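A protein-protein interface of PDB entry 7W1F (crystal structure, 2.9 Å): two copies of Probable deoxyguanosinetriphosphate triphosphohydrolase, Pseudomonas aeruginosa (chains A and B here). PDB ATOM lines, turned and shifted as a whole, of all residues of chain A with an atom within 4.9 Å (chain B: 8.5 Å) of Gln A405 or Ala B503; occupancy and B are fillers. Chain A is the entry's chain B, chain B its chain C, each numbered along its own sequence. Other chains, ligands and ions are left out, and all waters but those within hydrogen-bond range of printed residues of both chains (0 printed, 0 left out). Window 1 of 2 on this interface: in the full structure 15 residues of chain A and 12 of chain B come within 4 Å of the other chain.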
ATOM      1  N   THR A 401       8.526  30.014  14.115  1.00  0.00           N
ATOM      2  CA  THR A 401       8.785  29.195  12.935  1.00  0.00           C
ATOM      3  C   THR A 401      10.240  28.731  12.901  1.00  0.00           C
ATOM      4  O   THR A 401      10.529  27.577  12.556  1.00  0.00           O
ATOM      5  CB  THR A 401       8.418  29.960  11.667  1.00  0.00           C
ATOM      6  OG1 THR A 401       7.043  30.326  11.726  1.00  0.00           O
ATOM      7  CG2 THR A 401       8.616  29.101  10.455  1.00  0.00           C
ATOM      8  N   LEU A 402      11.176  29.624  13.231  1.00  0.00           N
ATOM      9  CA  LEU A 402      12.585  29.241  13.270  1.00  0.00           C
ATOM     10  C   LEU A 402      12.870  28.237  14.382  1.00  0.00           C
ATOM     11  O   LEU A 402      13.705  27.341  14.216  1.00  0.00           O
ATOM     12  CB  LEU A 402      13.462  30.473  13.435  1.00  0.00           C
ATOM     13  CG  LEU A 402      14.941  30.114  13.528  1.00  0.00           C
ATOM     14  CD1 LEU A 402      15.454  29.526  12.204  1.00  0.00           C
ATOM     15  CD2 LEU A 402      15.716  31.344  13.904  1.00  0.00           C
ATOM     16  N   GLU A 403      12.224  28.401  15.542  1.00  0.00           N
ATOM     17  CA  GLU A 403      12.402  27.437  16.623  1.00  0.00           C
ATOM     18  C   GLU A 403      11.937  26.052  16.183  1.00  0.00           C
ATOM     19  O   GLU A 403      12.667  25.063  16.313  1.00  0.00           O
ATOM     20  CB  GLU A 403      11.655  27.911  17.877  1.00  0.00           C
ATOM     21  CG  GLU A 403      12.114  29.283  18.395  1.00  0.00           C
ATOM     22  CD  GLU A 403      11.491  29.684  19.737  1.00  0.00           C
ATOM     23  OE1 GLU A 403      12.246  30.084  20.657  1.00  0.00           O
ATOM     24  OE2 GLU A 403      10.249  29.614  19.873  1.00  0.00           O
ATOM     25  N   LEU A 404      10.741  25.975  15.600  1.00  0.00           N
ATOM     26  CA  LEU A 404      10.232  24.698  15.116  1.00  0.00           C
ATOM     27  C   LEU A 404      11.098  24.131  13.993  1.00  0.00           C
ATOM     28  O   LEU A 404      11.384  22.930  13.963  1.00  0.00           O
ATOM     29  CB  LEU A 404       8.786  24.875  14.664  1.00  0.00           C
ATOM     30  CG  LEU A 404       7.895  23.643  14.657  1.00  0.00           C
ATOM     31  CD1 LEU A 404       8.079  22.889  15.945  1.00  0.00           C
ATOM     32  CD2 LEU A 404       6.452  24.096  14.518  1.00  0.00           C
ATOM     33  N   GLN A 405      11.525  24.974  13.053  1.00  0.00           N
ATOM     34  CA  GLN A 405      12.328  24.465  11.946  1.00  0.00           C
ATOM     35  C   GLN A 405      13.678  23.946  12.432  1.00  0.00           C
ATOM     36  O   GLN A 405      14.138  22.881  11.994  1.00  0.00           O
ATOM     37  CB  GLN A 405      12.505  25.543  10.898  1.00  0.00           C
ATOM     38  CG  GLN A 405      11.271  25.761  10.058  1.00  0.00           C
ATOM     39  CD  GLN A 405      11.476  26.850   9.009  1.00  0.00           C
ATOM     40  OE1 GLN A 405      12.477  27.572   9.024  1.00  0.00           O
ATOM     41  NE2 GLN A 405      10.513  26.993   8.123  1.00  0.00           N
ATOM     42  N   GLY A 406      14.338  24.690  13.321  1.00  0.00           N
ATOM     43  CA  GLY A 406      15.579  24.206  13.900  1.00  0.00           C
ATOM     44  C   GLY A 406      15.403  22.917  14.689  1.00  0.00           C
ATOM     45  O   GLY A 406      16.338  22.115  14.799  1.00  0.00           O
ATOM     46  N   TYR A 407      14.218  22.713  15.270  1.00  0.00           N
ATOM     47  CA  TYR A 407      13.942  21.453  15.944  1.00  0.00           C
ATOM     48  C   TYR A 407      14.052  20.284  14.975  1.00  0.00           C
ATOM     49  O   TYR A 407      14.622  19.243  15.318  1.00  0.00           O
ATOM     50  CB  TYR A 407      12.561  21.499  16.584  1.00  0.00           C
ATOM     51  CG  TYR A 407      12.265  20.377  17.555  1.00  0.00           C
ATOM     52  CD1 TYR A 407      11.538  19.260  17.166  1.00  0.00           C
ATOM     53  CD2 TYR A 407      12.698  20.448  18.876  1.00  0.00           C
ATOM     54  CE1 TYR A 407      11.252  18.253  18.061  1.00  0.00           C
ATOM     55  CE2 TYR A 407      12.422  19.443  19.771  1.00  0.00           C
ATOM     56  CZ  TYR A 407      11.697  18.351  19.359  1.00  0.00           C
ATOM     57  OH  TYR A 407      11.413  17.344  20.251  1.00  0.00           O
ATOM     58  N   ARG A 408      13.523  20.436  13.751  1.00  0.00           N
ATOM     59  CA  ARG A 408      13.624  19.356  12.769  1.00  0.00           C
ATOM     60  C   ARG A 408      15.065  19.144  12.345  1.00  0.00           C
ATOM     61  O   ARG A 408      15.525  18.003  12.230  1.00  0.00           O
ATOM     62  CB  ARG A 408      12.771  19.653  11.536  1.00  0.00           C
ATOM     63  CG  ARG A 408      11.411  19.026  11.555  1.00  0.00           C
ATOM     64  CD  ARG A 408      11.141  18.168  10.334  1.00  0.00           C
ATOM     65  NE  ARG A 408      12.289  17.348   9.977  1.00  0.00           N
ATOM     66  CZ  ARG A 408      12.697  16.297  10.672  1.00  0.00           C
ATOM     67  NH1 ARG A 408      13.752  15.597  10.279  1.00  0.00           N
ATOM     68  NH2 ARG A 408      12.049  15.954  11.771  1.00  0.00           N
ATOM     69  N   ILE A 409      15.796  20.237  12.124  1.00  0.00           N
ATOM     70  CA  ILE A 409      17.150  20.131  11.593  1.00  0.00           C
ATOM     71  C   ILE A 409      18.041  19.370  12.566  1.00  0.00           C
ATOM     72  O   ILE A 409      18.765  18.446  12.182  1.00  0.00           O
ATOM     73  CB  ILE A 409      17.712  21.530  11.290  1.00  0.00           C
ATOM     74  CG1 ILE A 409      16.851  22.213  10.234  1.00  0.00           C
ATOM     75  CG2 ILE A 409      19.147  21.432  10.816  1.00  0.00           C
ATOM     76  CD1 ILE A 409      17.113  23.699  10.106  1.00  0.00           C
ATOM     77  N   GLN A 495      21.413  23.961   8.822  1.00  0.00           N
ATOM     78  CA  GLN A 495      20.403  23.750   7.792  1.00  0.00           C
ATOM     79  C   GLN A 495      21.024  23.185   6.528  1.00  0.00           C
ATOM     80  O   GLN A 495      20.432  22.323   5.867  1.00  0.00           O
ATOM     81  CB  GLN A 495      19.674  25.048   7.475  1.00  0.00           C
ATOM     82  CG  GLN A 495      18.723  24.922   6.311  1.00  0.00           C
ATOM     83  CD  GLN A 495      17.337  25.373   6.686  1.00  0.00           C
ATOM     84  OE1 GLN A 495      17.177  26.264   7.523  1.00  0.00           O
ATOM     85  NE2 GLN A 495      16.323  24.757   6.089  1.00  0.00           N
ATOM     86  N   TYR A 498      21.768  19.465   6.871  1.00  0.00           N
ATOM     87  CA  TYR A 498      20.479  18.778   6.839  1.00  0.00           C
ATOM     88  C   TYR A 498      19.948  18.642   5.416  1.00  0.00           C
ATOM     89  O   TYR A 498      19.530  17.557   5.003  1.00  0.00           O
ATOM     90  CB  TYR A 498      19.478  19.540   7.711  1.00  0.00           C
ATOM     91  CG  TYR A 498      18.071  18.980   7.751  1.00  0.00           C
ATOM     92  CD1 TYR A 498      16.999  19.753   7.333  1.00  0.00           C
ATOM     93  CD2 TYR A 498      17.806  17.688   8.196  1.00  0.00           C
ATOM     94  CE1 TYR A 498      15.702  19.276   7.365  1.00  0.00           C
ATOM     95  CE2 TYR A 498      16.498  17.194   8.228  1.00  0.00           C
ATOM     96  CZ  TYR A 498      15.452  18.003   7.809  1.00  0.00           C
ATOM     97  OH  TYR A 498      14.144  17.565   7.818  1.00  0.00           O
ATOM     98  N   ARG A 499      19.976  19.732   4.645  1.00  0.00           N
ATOM     99  CA  ARG A 499      19.438  19.703   3.288  1.00  0.00           C
ATOM    100  C   ARG A 499      20.241  18.772   2.394  1.00  0.00           C
ATOM    101  O   ARG A 499      19.671  18.061   1.560  1.00  0.00           O
ATOM    102  CB  ARG A 499      19.382  21.117   2.715  1.00  0.00           C
ATOM    103  CG  ARG A 499      18.462  21.257   1.508  1.00  0.00           C
ATOM    104  CD  ARG A 499      18.407  22.687   0.983  1.00  0.00           C
ATOM    105  NE  ARG A 499      17.491  23.504   1.779  1.00  0.00           N
ATOM    106  CZ  ARG A 499      17.850  24.575   2.487  1.00  0.00           C
ATOM    107  NH1 ARG A 499      19.117  24.975   2.500  1.00  0.00           N
ATOM    108  NH2 ARG A 499      16.934  25.252   3.176  1.00  0.00           N
ATOM    109  N   PHE B 416       3.161  15.349  11.202  1.00  0.00           N
ATOM    110  CA  PHE B 416       3.768  16.502  11.866  1.00  0.00           C
ATOM    111  C   PHE B 416       2.977  16.944  13.097  1.00  0.00           C
ATOM    112  O   PHE B 416       3.571  17.367  14.098  1.00  0.00           O
ATOM    113  CB  PHE B 416       3.928  17.655  10.877  1.00  0.00           C
ATOM    114  CG  PHE B 416       5.243  17.656  10.141  1.00  0.00           C
ATOM    115  CD1 PHE B 416       6.438  17.539  10.834  1.00  0.00           C
ATOM    116  CD2 PHE B 416       5.293  17.790   8.767  1.00  0.00           C
ATOM    117  CE1 PHE B 416       7.654  17.549  10.173  1.00  0.00           C
ATOM    118  CE2 PHE B 416       6.511  17.797   8.100  1.00  0.00           C
ATOM    119  CZ  PHE B 416       7.696  17.674   8.811  1.00  0.00           C
ATOM    120  N   HIS B 441       7.647  22.074  22.458  1.00  0.00           N
ATOM    121  CA  HIS B 441       7.424  21.652  21.078  1.00  0.00           C
ATOM    122  C   HIS B 441       5.940  21.483  20.767  1.00  0.00           C
ATOM    123  O   HIS B 441       5.485  22.007  19.734  1.00  0.00           O
ATOM    124  CB  HIS B 441       8.213  20.377  20.786  1.00  0.00           C
ATOM    125  CG  HIS B 441       7.955  19.808  19.427  1.00  0.00           C
ATOM    126  ND1 HIS B 441       8.162  20.526  18.274  1.00  0.00           N
ATOM    127  CD2 HIS B 441       7.480  18.601  19.038  1.00  0.00           C
ATOM    128  CE1 HIS B 441       7.842  19.783  17.231  1.00  0.00           C
ATOM    129  NE2 HIS B 441       7.424  18.611  17.666  1.00  0.00           N
ATOM    130  N   LEU B 444       4.448  24.992  20.465  1.00  0.00           N
ATOM    131  CA  LEU B 444       4.633  25.628  19.163  1.00  0.00           C
ATOM    132  C   LEU B 444       3.654  25.074  18.141  1.00  0.00           C
ATOM    133  O   LEU B 444       3.118  25.825  17.316  1.00  0.00           O
ATOM    134  CB  LEU B 444       6.070  25.445  18.675  1.00  0.00           C
ATOM    135  CG  LEU B 444       7.180  26.244  19.353  1.00  0.00           C
ATOM    136  CD1 LEU B 444       8.436  26.167  18.520  1.00  0.00           C
ATOM    137  CD2 LEU B 444       6.766  27.683  19.554  1.00  0.00           C
ATOM    138  N   ARG B 448       0.402  27.277  16.097  1.00  0.00           N
ATOM    139  CA  ARG B 448       0.219  27.355  14.648  1.00  0.00           C
ATOM    140  C   ARG B 448      -1.216  27.072  14.209  1.00  0.00           C
ATOM    141  O   ARG B 448      -1.596  27.432  13.091  1.00  0.00           O
ATOM    142  CB  ARG B 448       1.161  26.375  13.958  1.00  0.00           C
ATOM    143  CG  ARG B 448       2.627  26.657  14.196  1.00  0.00           C
ATOM    144  CD  ARG B 448       3.453  25.747  13.298  1.00  0.00           C
ATOM    145  NE  ARG B 448       3.490  26.155  11.901  1.00  0.00           N
ATOM    146  CZ  ARG B 448       4.412  26.948  11.392  1.00  0.00           C
ATOM    147  NH1 ARG B 448       5.377  27.416  12.165  1.00  0.00           N
ATOM    148  NH2 ARG B 448       4.377  27.251  10.109  1.00  0.00           N
ATOM    149  N   ASP B 496       2.880  24.610   1.547  1.00  0.00           N
ATOM    150  CA  ASP B 496       3.734  25.516   2.303  1.00  0.00           C
ATOM    151  C   ASP B 496       3.957  24.995   3.715  1.00  0.00           C
ATOM    152  O   ASP B 496       5.101  24.867   4.167  1.00  0.00           O
ATOM    153  CB  ASP B 496       3.128  26.920   2.336  1.00  0.00           C
ATOM    154  CG  ASP B 496       3.348  27.683   1.043  1.00  0.00           C
ATOM    155  OD1 ASP B 496       4.014  27.140   0.124  1.00  0.00           O
ATOM    156  OD2 ASP B 496       2.833  28.824   0.947  1.00  0.00           O
ATOM    157  N   GLU B 497       2.867  24.665   4.419  1.00  0.00           N
ATOM    158  CA  GLU B 497       2.992  24.200   5.796  1.00  0.00           C
ATOM    159  C   GLU B 497       3.782  22.902   5.871  1.00  0.00           C
ATOM    160  O   GLU B 497       4.594  22.714   6.784  1.00  0.00           O
ATOM    161  CB  GLU B 497       1.616  24.036   6.429  1.00  0.00           C
ATOM    162  CG  GLU B 497       1.664  23.636   7.892  1.00  0.00           C
ATOM    163  CD  GLU B 497       2.158  24.746   8.810  1.00  0.00           C
ATOM    164  OE1 GLU B 497       2.306  24.489  10.019  1.00  0.00           O
ATOM    165  OE2 GLU B 497       2.405  25.868   8.338  1.00  0.00           O
ATOM    166  N   TYR B 498       3.556  21.998   4.919  1.00  0.00           N
ATOM    167  CA  TYR B 498       4.373  20.796   4.849  1.00  0.00           C
ATOM    168  C   TYR B 498       5.836  21.153   4.645  1.00  0.00           C
ATOM    169  O   TYR B 498       6.721  20.616   5.320  1.00  0.00           O
ATOM    170  CB  TYR B 498       3.885  19.881   3.727  1.00  0.00           C
ATOM    171  CG  TYR B 498       4.681  18.601   3.615  1.00  0.00           C
ATOM    172  CD1 TYR B 498       5.318  18.246   2.437  1.00  0.00           C
ATOM    173  CD2 TYR B 498       4.783  17.740   4.699  1.00  0.00           C
ATOM    174  CE1 TYR B 498       6.040  17.061   2.345  1.00  0.00           C
ATOM    175  CE2 TYR B 498       5.498  16.567   4.618  1.00  0.00           C
ATOM    176  CZ  TYR B 498       6.123  16.230   3.443  1.00  0.00           C
ATOM    177  OH  TYR B 498       6.834  15.056   3.378  1.00  0.00           O
ATOM    178  N   ARG B 499       6.105  22.060   3.708  1.00  0.00           N
ATOM    179  CA  ARG B 499       7.478  22.440   3.409  1.00  0.00           C
ATOM    180  C   ARG B 499       8.111  23.160   4.594  1.00  0.00           C
ATOM    181  O   ARG B 499       9.282  22.922   4.917  1.00  0.00           O
ATOM    182  CB  ARG B 499       7.521  23.292   2.130  1.00  0.00           C
ATOM    183  CG  ARG B 499       8.894  23.335   1.446  1.00  0.00           C
ATOM    184  CD  ARG B 499       8.939  24.187   0.169  1.00  0.00           C
ATOM    185  NE  ARG B 499       8.388  23.474  -0.984  1.00  0.00           N
ATOM    186  CZ  ARG B 499       7.317  23.871  -1.669  1.00  0.00           C
ATOM    187  NH1 ARG B 499       6.677  24.987  -1.325  1.00  0.00           N
ATOM    188  NH2 ARG B 499       6.884  23.156  -2.699  1.00  0.00           N
ATOM    189  N   ALA B 500       7.348  24.032   5.263  1.00  0.00           N
ATOM    190  CA  ALA B 500       7.900  24.811   6.367  1.00  0.00           C
ATOM    191  C   ALA B 500       8.320  23.912   7.515  1.00  0.00           C
ATOM    192  O   ALA B 500       9.454  23.995   8.001  1.00  0.00           O
ATOM    193  CB  ALA B 500       6.883  25.842   6.843  1.00  0.00           C
ATOM    194  N   LEU B 501       7.416  23.031   7.956  1.00  0.00           N
ATOM    195  CA  LEU B 501       7.735  22.130   9.058  1.00  0.00           C
ATOM    196  C   LEU B 501       8.860  21.176   8.695  1.00  0.00           C
ATOM    197  O   LEU B 501       9.654  20.795   9.564  1.00  0.00           O
ATOM    198  CB  LEU B 501       6.486  21.357   9.473  1.00  0.00           C
ATOM    199  CG  LEU B 501       5.360  22.220  10.045  1.00  0.00           C
ATOM    200  CD1 LEU B 501       4.314  21.306  10.645  1.00  0.00           C
ATOM    201  CD2 LEU B 501       5.864  23.241  11.066  1.00  0.00           C
ATOM    202  N   SER B 502       8.956  20.791   7.424  1.00  0.00           N
ATOM    203  CA  SER B 502      10.061  19.949   6.990  1.00  0.00           C
ATOM    204  C   SER B 502      11.393  20.663   7.099  1.00  0.00           C
ATOM    205  O   SER B 502      12.426  19.997   7.208  1.00  0.00           O
ATOM    206  CB  SER B 502       9.862  19.504   5.541  1.00  0.00           C
ATOM    207  OG  SER B 502       8.593  18.916   5.350  1.00  0.00           O
ATOM    208  N   ALA B 503      11.382  21.998   7.075  1.00  0.00           N
ATOM    209  CA  ALA B 503      12.589  22.821   7.130  1.00  0.00           C
ATOM    210  C   ALA B 503      13.486  22.584   5.917  1.00  0.00           C
ATOM    211  O   ALA B 503      14.712  22.646   6.019  1.00  0.00           O
ATOM    212  CB  ALA B 503      13.368  22.603   8.432  1.00  0.00           C
ATOM    213  N   LEU B 504      12.892  22.260   4.772  1.00  0.00           N
ATOM    214  CA  LEU B 504      13.668  22.132   3.542  1.00  0.00           C
ATOM    215  C   LEU B 504      13.228  23.165   2.491  1.00  0.00           C
ATOM    216  O   LEU B 504      13.808  24.255   2.378  1.00  0.00           O
ATOM    217  CB  LEU B 504      13.561  20.716   2.982  1.00  0.00           C
ATOM    218  CG  LEU B 504      14.254  19.621   3.801  1.00  0.00           C
ATOM    219  CD1 LEU B 504      14.037  18.254   3.182  1.00  0.00           C
ATOM    220  CD2 LEU B 504      15.729  19.918   3.934  1.00  0.00           C
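OG1 of Thr A401 is in hydrogen-bond range of NH1 of Arg B448, at 3.4 Å.
The side-chain amide nitrogen of Gln A405 sits at hydrogen-bond distance from the backbone carbonyl oxygen of Ala B500, 3.2 Å away.
O of Ala B503 is in hydrogen-bond range of NE2 of Gln A495.
The side-chain hydroxyl of Tyr A498 is in hydrogen-bond range of the backbone carbonyl oxygen of Ser B502.
The backbone carbonyl oxygen (O) of Leu B504 lies within hydrogen-bond range of the guanidinium group (NH2) of Arg A499 (3.4 Å).
NE of Arg A408 is in hydrogen-bond range of OH of Tyr A498 (2.9 Å).
The side-chain amide nitrogen (NE2) of Gln A495 lies close to the guanidinium group (NH2) of Arg A499 (3.0 Å).
OE1 of Glu B497 lies within salt-bridge range of NE of Arg B448, at 2.8 Å.
The side-chain hydroxyl (OG) of Ser B502 sits at hydrogen-bond distance from the backbone carbonyl oxygen (O) of Tyr B498, 2.5 Å away.
Among the printed residues, pairs that only touch across the chains: Glu A403 with Leu B444 (3.7 Å), Leu A404 with His B441 (3.3 Å), Leu A404 with Leu B444 (3.7 Å), Leu A404 with Arg B448 (3.6 Å), Leu A404 with Leu B501 (3.6 Å), Gln A405 with Ala B503 (3.7 Å), Tyr A407 with His B441 (3.7 Å), Arg A408 with Phe B416 (3.5 Å), Arg A408 with Leu B501 (3.1 Å), Arg A408 with Ser B502 (3.8 Å), Ile A409 with Ala B503 (3.9 Å), Tyr A498 with Ala B503 (3.8 Å) and Tyr A498 with Leu B504 (3.5 Å).
Printed residues of chain B within 4 Å of Thr A401: Arg B448 (3.4 Å).
Of the printed residues of chain B, Glu A403 touches Leu B444 (3.7 Å).
Of the printed residues of chain B, Arg A408 touches Phe B416, Leu B501 and Ser B502.
Of the printed residues of chain A, Phe B416 touches Arg A408 (3.5 Å).
Of the printed residues of chain A, Leu B501 touches Leu A404 (3.6 Å) and Arg A408 (3.1 Å).
Ala B503 touches four residues of chain A.
The nearest residue of chain A that does not touch Ala B503 is Arg A408 (4.3 Å).
The nearest printed residue of chain B that does not touch Arg A499 is Ala B503 (4.5 Å).
Of the 12 printed residues of chain A, 10 touch a printed residue of chain B.
Hydrophobic or aromatic side chains of chain A that line the printed part of chain B: Leu A404, Tyr A407, Ile A409 and Tyr A498.
Of the 13 printed residues of chain B, 9 touch a printed residue of chain A.
Hydrophobic or aromatic side chains of chain B within 4 Å of the printed part of chain A: Phe B416, His B441, Leu B444, Leu B501, Ala B503 and Leu B504.
Among the printed residues, 18 pairs touch across the chains.
2 positions are printed for both chains.
Of the 18 pairs that touch across the chains among the printed residues, none has its exchanged pair printed and touching as well.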
